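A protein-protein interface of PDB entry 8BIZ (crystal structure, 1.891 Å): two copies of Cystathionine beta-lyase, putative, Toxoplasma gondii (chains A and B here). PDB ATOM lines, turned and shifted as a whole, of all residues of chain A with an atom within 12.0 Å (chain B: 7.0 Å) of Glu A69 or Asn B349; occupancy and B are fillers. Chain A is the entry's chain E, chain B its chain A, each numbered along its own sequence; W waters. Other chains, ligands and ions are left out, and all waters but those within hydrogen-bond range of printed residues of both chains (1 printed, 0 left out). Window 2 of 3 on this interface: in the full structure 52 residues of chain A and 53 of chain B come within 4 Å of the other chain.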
ATOM      1  N   VAL A  64      11.528   4.436  22.356  1.00  0.00           N
ATOM      2  CA  VAL A  64      12.855   3.951  22.015  1.00  0.00           C
ATOM      3  C   VAL A  64      13.718   5.126  21.575  1.00  0.00           C
ATOM      4  O   VAL A  64      13.245   6.036  20.880  1.00  0.00           O
ATOM      5  CB  VAL A  64      12.742   2.867  20.930  1.00  0.00           C
ATOM      6  CG1 VAL A  64      14.096   2.335  20.535  1.00  0.00           C
ATOM      7  CG2 VAL A  64      11.833   1.731  21.411  1.00  0.00           C
ATOM      8  N   GLN A  65      14.986   5.114  21.986  1.00  0.00           N
ATOM      9  CA  GLN A  65      15.945   6.170  21.689  1.00  0.00           C
ATOM     10  C   GLN A  65      16.902   5.711  20.596  1.00  0.00           C
ATOM     11  O   GLN A  65      17.303   4.543  20.563  1.00  0.00           O
ATOM     12  CB  GLN A  65      16.728   6.545  22.947  1.00  0.00           C
ATOM     13  CG  GLN A  65      15.818   6.807  24.142  1.00  0.00           C
ATOM     14  CD  GLN A  65      14.952   8.037  23.941  1.00  0.00           C
ATOM     15  OE1 GLN A  65      15.385   9.013  23.326  1.00  0.00           O
ATOM     16  NE2 GLN A  65      13.707   7.975  24.408  1.00  0.00           N
ATOM     17  N   GLU A  66      17.266   6.637  19.699  1.00  0.00           N
ATOM     18  CA  GLU A  66      18.126   6.274  18.573  1.00  0.00           C
ATOM     19  C   GLU A  66      19.522   5.877  19.036  1.00  0.00           C
ATOM     20  O   GLU A  66      20.133   4.959  18.477  1.00  0.00           O
ATOM     21  CB  GLU A  66      18.210   7.433  17.572  1.00  0.00           C
ATOM     22  CG  GLU A  66      18.608   7.009  16.168  1.00  0.00           C
ATOM     23  CD  GLU A  66      18.815   8.182  15.217  1.00  0.00           C
ATOM     24  OE1 GLU A  66      18.967   7.937  13.992  1.00  0.00           O
ATOM     25  OE2 GLU A  66      18.827   9.342  15.694  1.00  0.00           O
ATOM     26  N   SER A  67      20.045   6.552  20.052  1.00  0.00           N
ATOM     27  CA  SER A  67      21.373   6.256  20.570  1.00  0.00           C
ATOM     28  C   SER A  67      21.507   6.950  21.912  1.00  0.00           C
ATOM     29  O   SER A  67      20.630   7.715  22.322  1.00  0.00           O
ATOM     30  CB  SER A  67      22.471   6.710  19.604  1.00  0.00           C
ATOM     31  OG  SER A  67      22.447   8.121  19.421  1.00  0.00           O
ATOM     32  N   VAL A  68      22.620   6.680  22.599  1.00  0.00           N
ATOM     33  CA  VAL A  68      22.869   7.367  23.860  1.00  0.00           C
ATOM     34  C   VAL A  68      23.049   8.864  23.624  1.00  0.00           C
ATOM     35  O   VAL A  68      22.684   9.678  24.480  1.00  0.00           O
ATOM     36  CB  VAL A  68      24.089   6.751  24.574  1.00  0.00           C
ATOM     37  CG1 VAL A  68      24.307   7.404  25.933  1.00  0.00           C
ATOM     38  CG2 VAL A  68      23.909   5.252  24.732  1.00  0.00           C
ATOM     39  N   GLU A  69      23.579   9.258  22.461  1.00  0.00           N
ATOM     40  CA  GLU A  69      23.830  10.674  22.190  1.00  0.00           C
ATOM     41  C   GLU A  69      22.567  11.402  21.735  1.00  0.00           C
ATOM     42  O   GLU A  69      22.325  12.545  22.148  1.00  0.00           O
ATOM     43  CB  GLU A  69      24.934  10.851  21.140  1.00  0.00           C
ATOM     44  CG  GLU A  69      26.165   9.955  21.315  1.00  0.00           C
ATOM     45  CD  GLU A  69      25.927   8.510  20.898  1.00  0.00           C
ATOM     46  OE1 GLU A  69      25.806   8.230  19.687  1.00  0.00           O
ATOM     47  OE2 GLU A  69      25.834   7.660  21.806  1.00  0.00           O
ATOM     48  N   ASN A  70      21.752  10.771  20.887  1.00  0.00           N
ATOM     49  CA  ASN A  70      20.485  11.373  20.474  1.00  0.00           C
ATOM     50  C   ASN A  70      19.344  10.987  21.406  1.00  0.00           C
ATOM     51  O   ASN A  70      18.235  10.694  20.969  1.00  0.00           O
ATOM     52  CB  ASN A  70      20.179  11.001  19.031  1.00  0.00           C
ATOM     53  CG  ASN A  70      21.091  11.696  18.058  1.00  0.00           C
ATOM     54  OD1 ASN A  70      21.922  12.507  18.459  1.00  0.00           O
ATOM     55  ND2 ASN A  70      20.919  11.422  16.771  1.00  0.00           N
ATOM     56  N   TYR A  71      19.616  11.023  22.710  1.00  0.00           N
ATOM     57  CA  TYR A  71      18.598  10.789  23.723  1.00  0.00           C
ATOM     58  C   TYR A  71      17.645  11.978  23.782  1.00  0.00           C
ATOM     59  O   TYR A  71      18.087  13.131  23.815  1.00  0.00           O
ATOM     60  CB  TYR A  71      19.261  10.554  25.081  1.00  0.00           C
ATOM     61  CG  TYR A  71      18.325  10.452  26.259  1.00  0.00           C
ATOM     62  CD1 TYR A  71      17.299   9.513  26.289  1.00  0.00           C
ATOM     63  CD2 TYR A  71      18.477  11.291  27.355  1.00  0.00           C
ATOM     64  CE1 TYR A  71      16.443   9.421  27.378  1.00  0.00           C
ATOM     65  CE2 TYR A  71      17.630  11.205  28.445  1.00  0.00           C
ATOM     66  CZ  TYR A  71      16.614  10.271  28.454  1.00  0.00           C
ATOM     67  OH  TYR A  71      15.771  10.191  29.540  1.00  0.00           O
ATOM     68  N   LEU A  72      16.337  11.691  23.793  1.00  0.00           N
ATOM     69  CA  LEU A  72      15.280  12.706  23.753  1.00  0.00           C
ATOM     70  C   LEU A  72      15.300  13.507  22.450  1.00  0.00           C
ATOM     71  O   LEU A  72      14.692  14.575  22.364  1.00  0.00           O
ATOM     72  CB  LEU A  72      15.355  13.636  24.969  1.00  0.00           C
ATOM     73  CG  LEU A  72      14.857  13.021  26.288  1.00  0.00           C
ATOM     74  CD1 LEU A  72      15.261  13.853  27.512  1.00  0.00           C
ATOM     75  CD2 LEU A  72      13.335  12.840  26.235  1.00  0.00           C
ATOM     76  N   SER A  73      15.955  12.981  21.405  1.00  0.00           N
ATOM     77  CA  SER A  73      16.008  13.708  20.139  1.00  0.00           C
ATOM     78  C   SER A  73      14.630  13.808  19.494  1.00  0.00           C
ATOM     79  O   SER A  73      14.348  14.784  18.791  1.00  0.00           O
ATOM     80  CB  SER A  73      16.990  13.063  19.154  1.00  0.00           C
ATOM     81  OG  SER A  73      16.616  11.739  18.771  1.00  0.00           O
ATOM     82  N   LYS A  74      13.763  12.814  19.706  1.00  0.00           N
ATOM     83  CA  LYS A  74      12.414  12.857  19.161  1.00  0.00           C
ATOM     84  C   LYS A  74      11.397  13.389  20.166  1.00  0.00           C
ATOM     85  O   LYS A  74      10.198  13.401  19.870  1.00  0.00           O
ATOM     86  CB  LYS A  74      12.005  11.470  18.657  1.00  0.00           C
ATOM     87  CG  LYS A  74      12.918  10.945  17.547  1.00  0.00           C
ATOM     88  CD  LYS A  74      12.382   9.668  16.904  1.00  0.00           C
ATOM     89  CE  LYS A  74      13.413   9.074  15.958  1.00  0.00           C
ATOM     90  NZ  LYS A  74      12.859   7.973  15.096  1.00  0.00           N
ATOM     91  N   GLY A  75      11.842  13.815  21.346  1.00  0.00           N
ATOM     92  CA  GLY A  75      11.024  14.570  22.268  1.00  0.00           C
ATOM     93  C   GLY A  75      10.366  13.788  23.382  1.00  0.00           C
ATOM     94  O   GLY A  75       9.772  14.409  24.264  1.00  0.00           O
ATOM     95  N   PHE A  76      10.441  12.456  23.383  1.00  0.00           N
ATOM     96  CA  PHE A  76       9.716  11.674  24.379  1.00  0.00           C
ATOM     97  C   PHE A  76      10.606  10.574  24.940  1.00  0.00           C
ATOM     98  O   PHE A  76      11.551  10.124  24.285  1.00  0.00           O
ATOM     99  CB  PHE A  76       8.432  11.080  23.779  1.00  0.00           C
ATOM    100  CG  PHE A  76       7.487  12.125  23.268  1.00  0.00           C
ATOM    101  CD1 PHE A  76       6.569  12.718  24.125  1.00  0.00           C
ATOM    102  CD2 PHE A  76       7.555  12.557  21.951  1.00  0.00           C
ATOM    103  CE1 PHE A  76       5.721  13.711  23.674  1.00  0.00           C
ATOM    104  CE2 PHE A  76       6.702  13.553  21.484  1.00  0.00           C
ATOM    105  CZ  PHE A  76       5.786  14.129  22.350  1.00  0.00           C
ATOM    106  N   SER A  77      10.294  10.153  26.169  1.00  0.00           N
ATOM    107  CA  SER A  77      11.039   9.078  26.812  1.00  0.00           C
ATOM    108  C   SER A  77      10.123   8.185  27.637  1.00  0.00           C
ATOM    109  O   SER A  77      10.308   6.966  27.655  1.00  0.00           O
ATOM    110  CB  SER A  77      12.143   9.630  27.708  1.00  0.00           C
ATOM    111  OG  SER A  77      11.600  10.504  28.690  1.00  0.00           O
ATOM    112  N   ALA B 343      33.077   1.962  26.327  1.00  0.00           N
ATOM    113  CA  ALA B 343      32.671   0.631  25.880  1.00  0.00           C
ATOM    114  C   ALA B 343      31.185   0.396  26.131  1.00  0.00           C
ATOM    115  O   ALA B 343      30.492  -0.198  25.299  1.00  0.00           O
ATOM    116  CB  ALA B 343      33.515  -0.435  26.576  1.00  0.00           C
ATOM    117  N   GLY B 344      30.674   0.868  27.270  1.00  0.00           N
ATOM    118  CA  GLY B 344      29.254   0.716  27.548  1.00  0.00           C
ATOM    119  C   GLY B 344      28.392   1.479  26.565  1.00  0.00           C
ATOM    120  O   GLY B 344      27.360   0.981  26.107  1.00  0.00           O
ATOM    121  N   ILE B 345      28.806   2.706  26.229  1.00  0.00           N
ATOM    122  CA  ILE B 345      28.070   3.518  25.260  1.00  0.00           C
ATOM    123  C   ILE B 345      28.075   2.849  23.894  1.00  0.00           C
ATOM    124  O   ILE B 345      27.056   2.818  23.191  1.00  0.00           O
ATOM    125  CB  ILE B 345      28.665   4.938  25.190  1.00  0.00           C
ATOM    126  CG1 ILE B 345      28.339   5.701  26.470  1.00  0.00           C
ATOM    127  CG2 ILE B 345      28.177   5.665  23.947  1.00  0.00           C
ATOM    128  CD1 ILE B 345      29.108   7.005  26.631  1.00  0.00           C
ATOM    129  N   ARG B 346      29.234   2.338  23.477  1.00  0.00           N
ATOM    130  CA  ARG B 346      29.312   1.700  22.169  1.00  0.00           C
ATOM    131  C   ARG B 346      28.460   0.430  22.132  1.00  0.00           C
ATOM    132  O   ARG B 346      27.770   0.149  21.139  1.00  0.00           O
ATOM    133  CB  ARG B 346      30.774   1.404  21.847  1.00  0.00           C
ATOM    134  CG  ARG B 346      31.067   1.125  20.405  1.00  0.00           C
ATOM    135  CD  ARG B 346      32.557   1.246  20.160  1.00  0.00           C
ATOM    136  NE  ARG B 346      33.037   0.191  19.282  1.00  0.00           N
ATOM    137  CZ  ARG B 346      32.848   0.201  17.970  1.00  0.00           C
ATOM    138  NH1 ARG B 346      32.172   1.206  17.403  1.00  0.00           N
ATOM    139  NH2 ARG B 346      33.331  -0.793  17.238  1.00  0.00           N
ATOM    140  N   MET B 347      28.457  -0.328  23.226  1.00  0.00           N
ATOM    141  CA  MET B 347      27.599  -1.505  23.292  1.00  0.00           C
ATOM    142  C   MET B 347      26.127  -1.113  23.174  1.00  0.00           C
ATOM    143  O   MET B 347      25.365  -1.754  22.442  1.00  0.00           O
ATOM    144  CB  MET B 347      27.861  -2.255  24.592  1.00  0.00           C
ATOM    145  CG  MET B 347      27.125  -3.559  24.663  1.00  0.00           C
ATOM    146  SD  MET B 347      26.120  -3.568  26.136  1.00  0.00           S
ATOM    147  CE  MET B 347      24.669  -2.700  25.575  1.00  0.00           C
ATOM    148  N   MET B 348      25.713  -0.051  23.874  1.00  0.00           N
ATOM    149  CA  MET B 348      24.337   0.435  23.753  1.00  0.00           C
ATOM    150  C   MET B 348      24.002   0.811  22.326  1.00  0.00           C
ATOM    151  O   MET B 348      22.950   0.433  21.799  1.00  0.00           O
ATOM    152  CB  MET B 348      24.128   1.650  24.649  1.00  0.00           C
ATOM    153  CG  MET B 348      24.184   1.271  26.060  1.00  0.00           C
ATOM    154  SD  MET B 348      22.932   0.046  26.423  1.00  0.00           S
ATOM    155  CE  MET B 348      22.947   0.379  28.163  1.00  0.00           C
ATOM    156  N   ASN B 349      24.859   1.608  21.700  1.00  0.00           N
ATOM    157  CA  ASN B 349      24.576   2.039  20.344  1.00  0.00           C
ATOM    158  C   ASN B 349      24.552   0.884  19.359  1.00  0.00           C
ATOM    159  O   ASN B 349      24.049   1.066  18.245  1.00  0.00           O
ATOM    160  CB  ASN B 349      25.594   3.091  19.921  1.00  0.00           C
ATOM    161  CG  ASN B 349      25.467   4.349  20.734  1.00  0.00           C
ATOM    162  OD1 ASN B 349      24.458   4.548  21.415  1.00  0.00           O
ATOM    163  ND2 ASN B 349      26.477   5.210  20.676  1.00  0.00           N
ATOM    164  N   HIS B 350      25.067  -0.293  19.727  1.00  0.00           N
ATOM    165  CA  HIS B 350      25.078  -1.391  18.777  1.00  0.00           C
ATOM    166  C   HIS B 350      24.189  -2.577  19.146  1.00  0.00           C
ATOM    167  O   HIS B 350      24.271  -3.609  18.477  1.00  0.00           O
ATOM    168  CB  HIS B 350      26.521  -1.856  18.574  1.00  0.00           C
ATOM    169  CG  HIS B 350      27.354  -0.871  17.818  1.00  0.00           C
ATOM    170  ND1 HIS B 350      28.022   0.165  18.435  1.00  0.00           N
ATOM    171  CD2 HIS B 350      27.641  -0.772  16.499  1.00  0.00           C
ATOM    172  CE1 HIS B 350      28.677   0.868  17.526  1.00  0.00           C
ATOM    173  NE2 HIS B 350      28.466   0.316  16.344  1.00  0.00           N
ATOM    174  N   VAL B 351      23.328  -2.477  20.156  1.00  0.00           N
ATOM    175  CA  VAL B 351      22.509  -3.642  20.488  1.00  0.00           C
ATOM    176  C   VAL B 351      21.338  -3.704  19.509  1.00  0.00           C
ATOM    177  O   VAL B 351      20.577  -2.734  19.382  1.00  0.00           O
ATOM    178  CB  VAL B 351      22.083  -3.626  21.965  1.00  0.00           C
ATOM    179  CG1 VAL B 351      21.223  -2.420  22.282  1.00  0.00           C
ATOM    180  CG2 VAL B 351      21.375  -4.922  22.327  1.00  0.00           C
ATOM    181  N   PRO B 352      21.179  -4.791  18.765  1.00  0.00           N
ATOM    182  CA  PRO B 352      20.155  -4.825  17.723  1.00  0.00           C
ATOM    183  C   PRO B 352      18.807  -5.284  18.259  1.00  0.00           C
ATOM    184  O   PRO B 352      18.669  -5.726  19.396  1.00  0.00           O
ATOM    185  CB  PRO B 352      20.720  -5.833  16.722  1.00  0.00           C
ATOM    186  CG  PRO B 352      21.405  -6.818  17.595  1.00  0.00           C
ATOM    187  CD  PRO B 352      21.965  -6.038  18.779  1.00  0.00           C
ATOM    188  N   LEU B 357      16.193   0.010  23.109  1.00  0.00           N
ATOM    189  CA  LEU B 357      16.971   0.946  23.924  1.00  0.00           C
ATOM    190  C   LEU B 357      16.031   2.025  24.448  1.00  0.00           C
ATOM    191  O   LEU B 357      15.636   2.926  23.709  1.00  0.00           O
ATOM    192  CB  LEU B 357      18.107   1.548  23.099  1.00  0.00           C
ATOM    193  CG  LEU B 357      19.087   2.523  23.760  1.00  0.00           C
ATOM    194  CD1 LEU B 357      19.919   1.826  24.822  1.00  0.00           C
ATOM    195  CD2 LEU B 357      20.002   3.132  22.698  1.00  0.00           C
ATOM    196  N   PHE B 374      19.624   7.805  31.741  1.00  0.00           N
ATOM    197  CA  PHE B 374      18.206   7.632  31.458  1.00  0.00           C
ATOM    198  C   PHE B 374      17.343   7.870  32.693  1.00  0.00           C
ATOM    199  O   PHE B 374      16.261   8.469  32.597  1.00  0.00           O
ATOM    200  CB  PHE B 374      17.973   6.225  30.891  1.00  0.00           C
ATOM    201  CG  PHE B 374      18.255   6.095  29.407  1.00  0.00           C
ATOM    202  CD1 PHE B 374      17.343   5.443  28.586  1.00  0.00           C
ATOM    203  CD2 PHE B 374      19.429   6.595  28.834  1.00  0.00           C
ATOM    204  CE1 PHE B 374      17.586   5.278  27.231  1.00  0.00           C
ATOM    205  CE2 PHE B 374      19.670   6.448  27.477  1.00  0.00           C
ATOM    206  CZ  PHE B 374      18.749   5.790  26.675  1.00  0.00           C
ATOM    207  N   ALA B 413      26.435  -7.074  20.176  1.00  0.00           N
ATOM    208  CA  ALA B 413      26.739  -5.768  20.758  1.00  0.00           C
ATOM    209  C   ALA B 413      28.029  -5.798  21.579  1.00  0.00           C
ATOM    210  O   ALA B 413      28.821  -4.851  21.540  1.00  0.00           O
ATOM    211  CB  ALA B 413      25.570  -5.298  21.621  1.00  0.00           C
HETATM  212  O   HOH W   1      22.924   3.809  17.926  1.00  0.00           O
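Hydrophobic or aromatic side chains of chain A that line the printed part of chain B: Val A64, Val A68 and Tyr A71.
Hydrophobic or aromatic side chains of chain B within 4 Å of the printed part of chain A: Ile B345, Met B348, Leu B357 and Phe B374.
Among the printed residues, 9 pairs touch across the chains.
Among the printed residues, no Asp or Glu carboxylate lies within 4 Å of a Lys or Arg side-chain nitrogen of the other chain.
Among the printed residues, pairs that only touch across the chains: Val A64 with Leu B357, Gln A65 with Phe B374, Ser A67 with Asn B349, Val A68 with Met B348, Glu A69 with Ile B345 and Tyr A71 with Phe B374.
No position is printed for both chains.
The side-chain hydroxyl (OG) of Ser A67 is in hydrogen-bond range of the backbone NH (N) of Asn A70 (3.1 Å).
The backbone NH (N) of Leu A72 is in hydrogen-bond range of the side-chain amide oxygen (OE1) of Gln A65 (2.9 Å).
The side-chain amide nitrogen of Gln A65 lies within hydrogen-bond range of the backbone carbonyl oxygen of Phe A76 (3.0 Å).
The side-chain hydroxyl (OG) of Ser A67 lies within hydrogen-bond range of the side-chain carboxylate (OE1) of Glu A69, 3.4 Å away.
The side-chain carboxylate (OE2) of Glu A69 sits at hydrogen-bond distance from the side-chain amide nitrogen (ND2) of Asn B349 (2.8 Å).
The backbone NH (N) of Val A68 sits at hydrogen-bond distance from the side-chain amide oxygen (OD1) of Asn B349, at 3.1 Å.
N of Gln A65 sits at hydrogen-bond distance from O of Leu B357 (2.9 Å).
Glu A69 touches just these residues of chain B: Ile B345 (3.7 Å) and Asn B349 (2.8 Å).
Of chain A, only Ser A67 (3.4 Å), Val A68 (3.1 Å) and Glu A69 (2.8 Å) come within 4 Å of Asn B349.
Met B347 touches none of the printed residues of chain A.
Printed residues of chain A within 4 Å of Met B348: Val A68.
His B350 touches none of the printed residues of chain A.
Printed residues of chain A within 4 Å of Leu B357: Val A64 (3.4 Å) and Gln A65 (2.9 Å).
Printed residues of chain B within 4 Å of Val A64: Leu B357 (3.4 Å).
Of the printed residues of chain B, Ser A67 touches Asn B349.
The nearest residue of chain B that does not touch Glu A69 is Arg B346 (6.5 Å).
The nearest residue of chain A that does not touch Asn B349 is Glu A66 (5.2 Å).
The nearest printed residue of chain B that does not touch Ser A67 is Leu B357 (4.02 Å).
Water W1 lies within hydrogen-bond range of the backbone carbonyl oxygen (O) of Asn B349 (3.0 Å) and the backbone carbonyl oxygen (O) of Glu A66 (3.1 Å).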
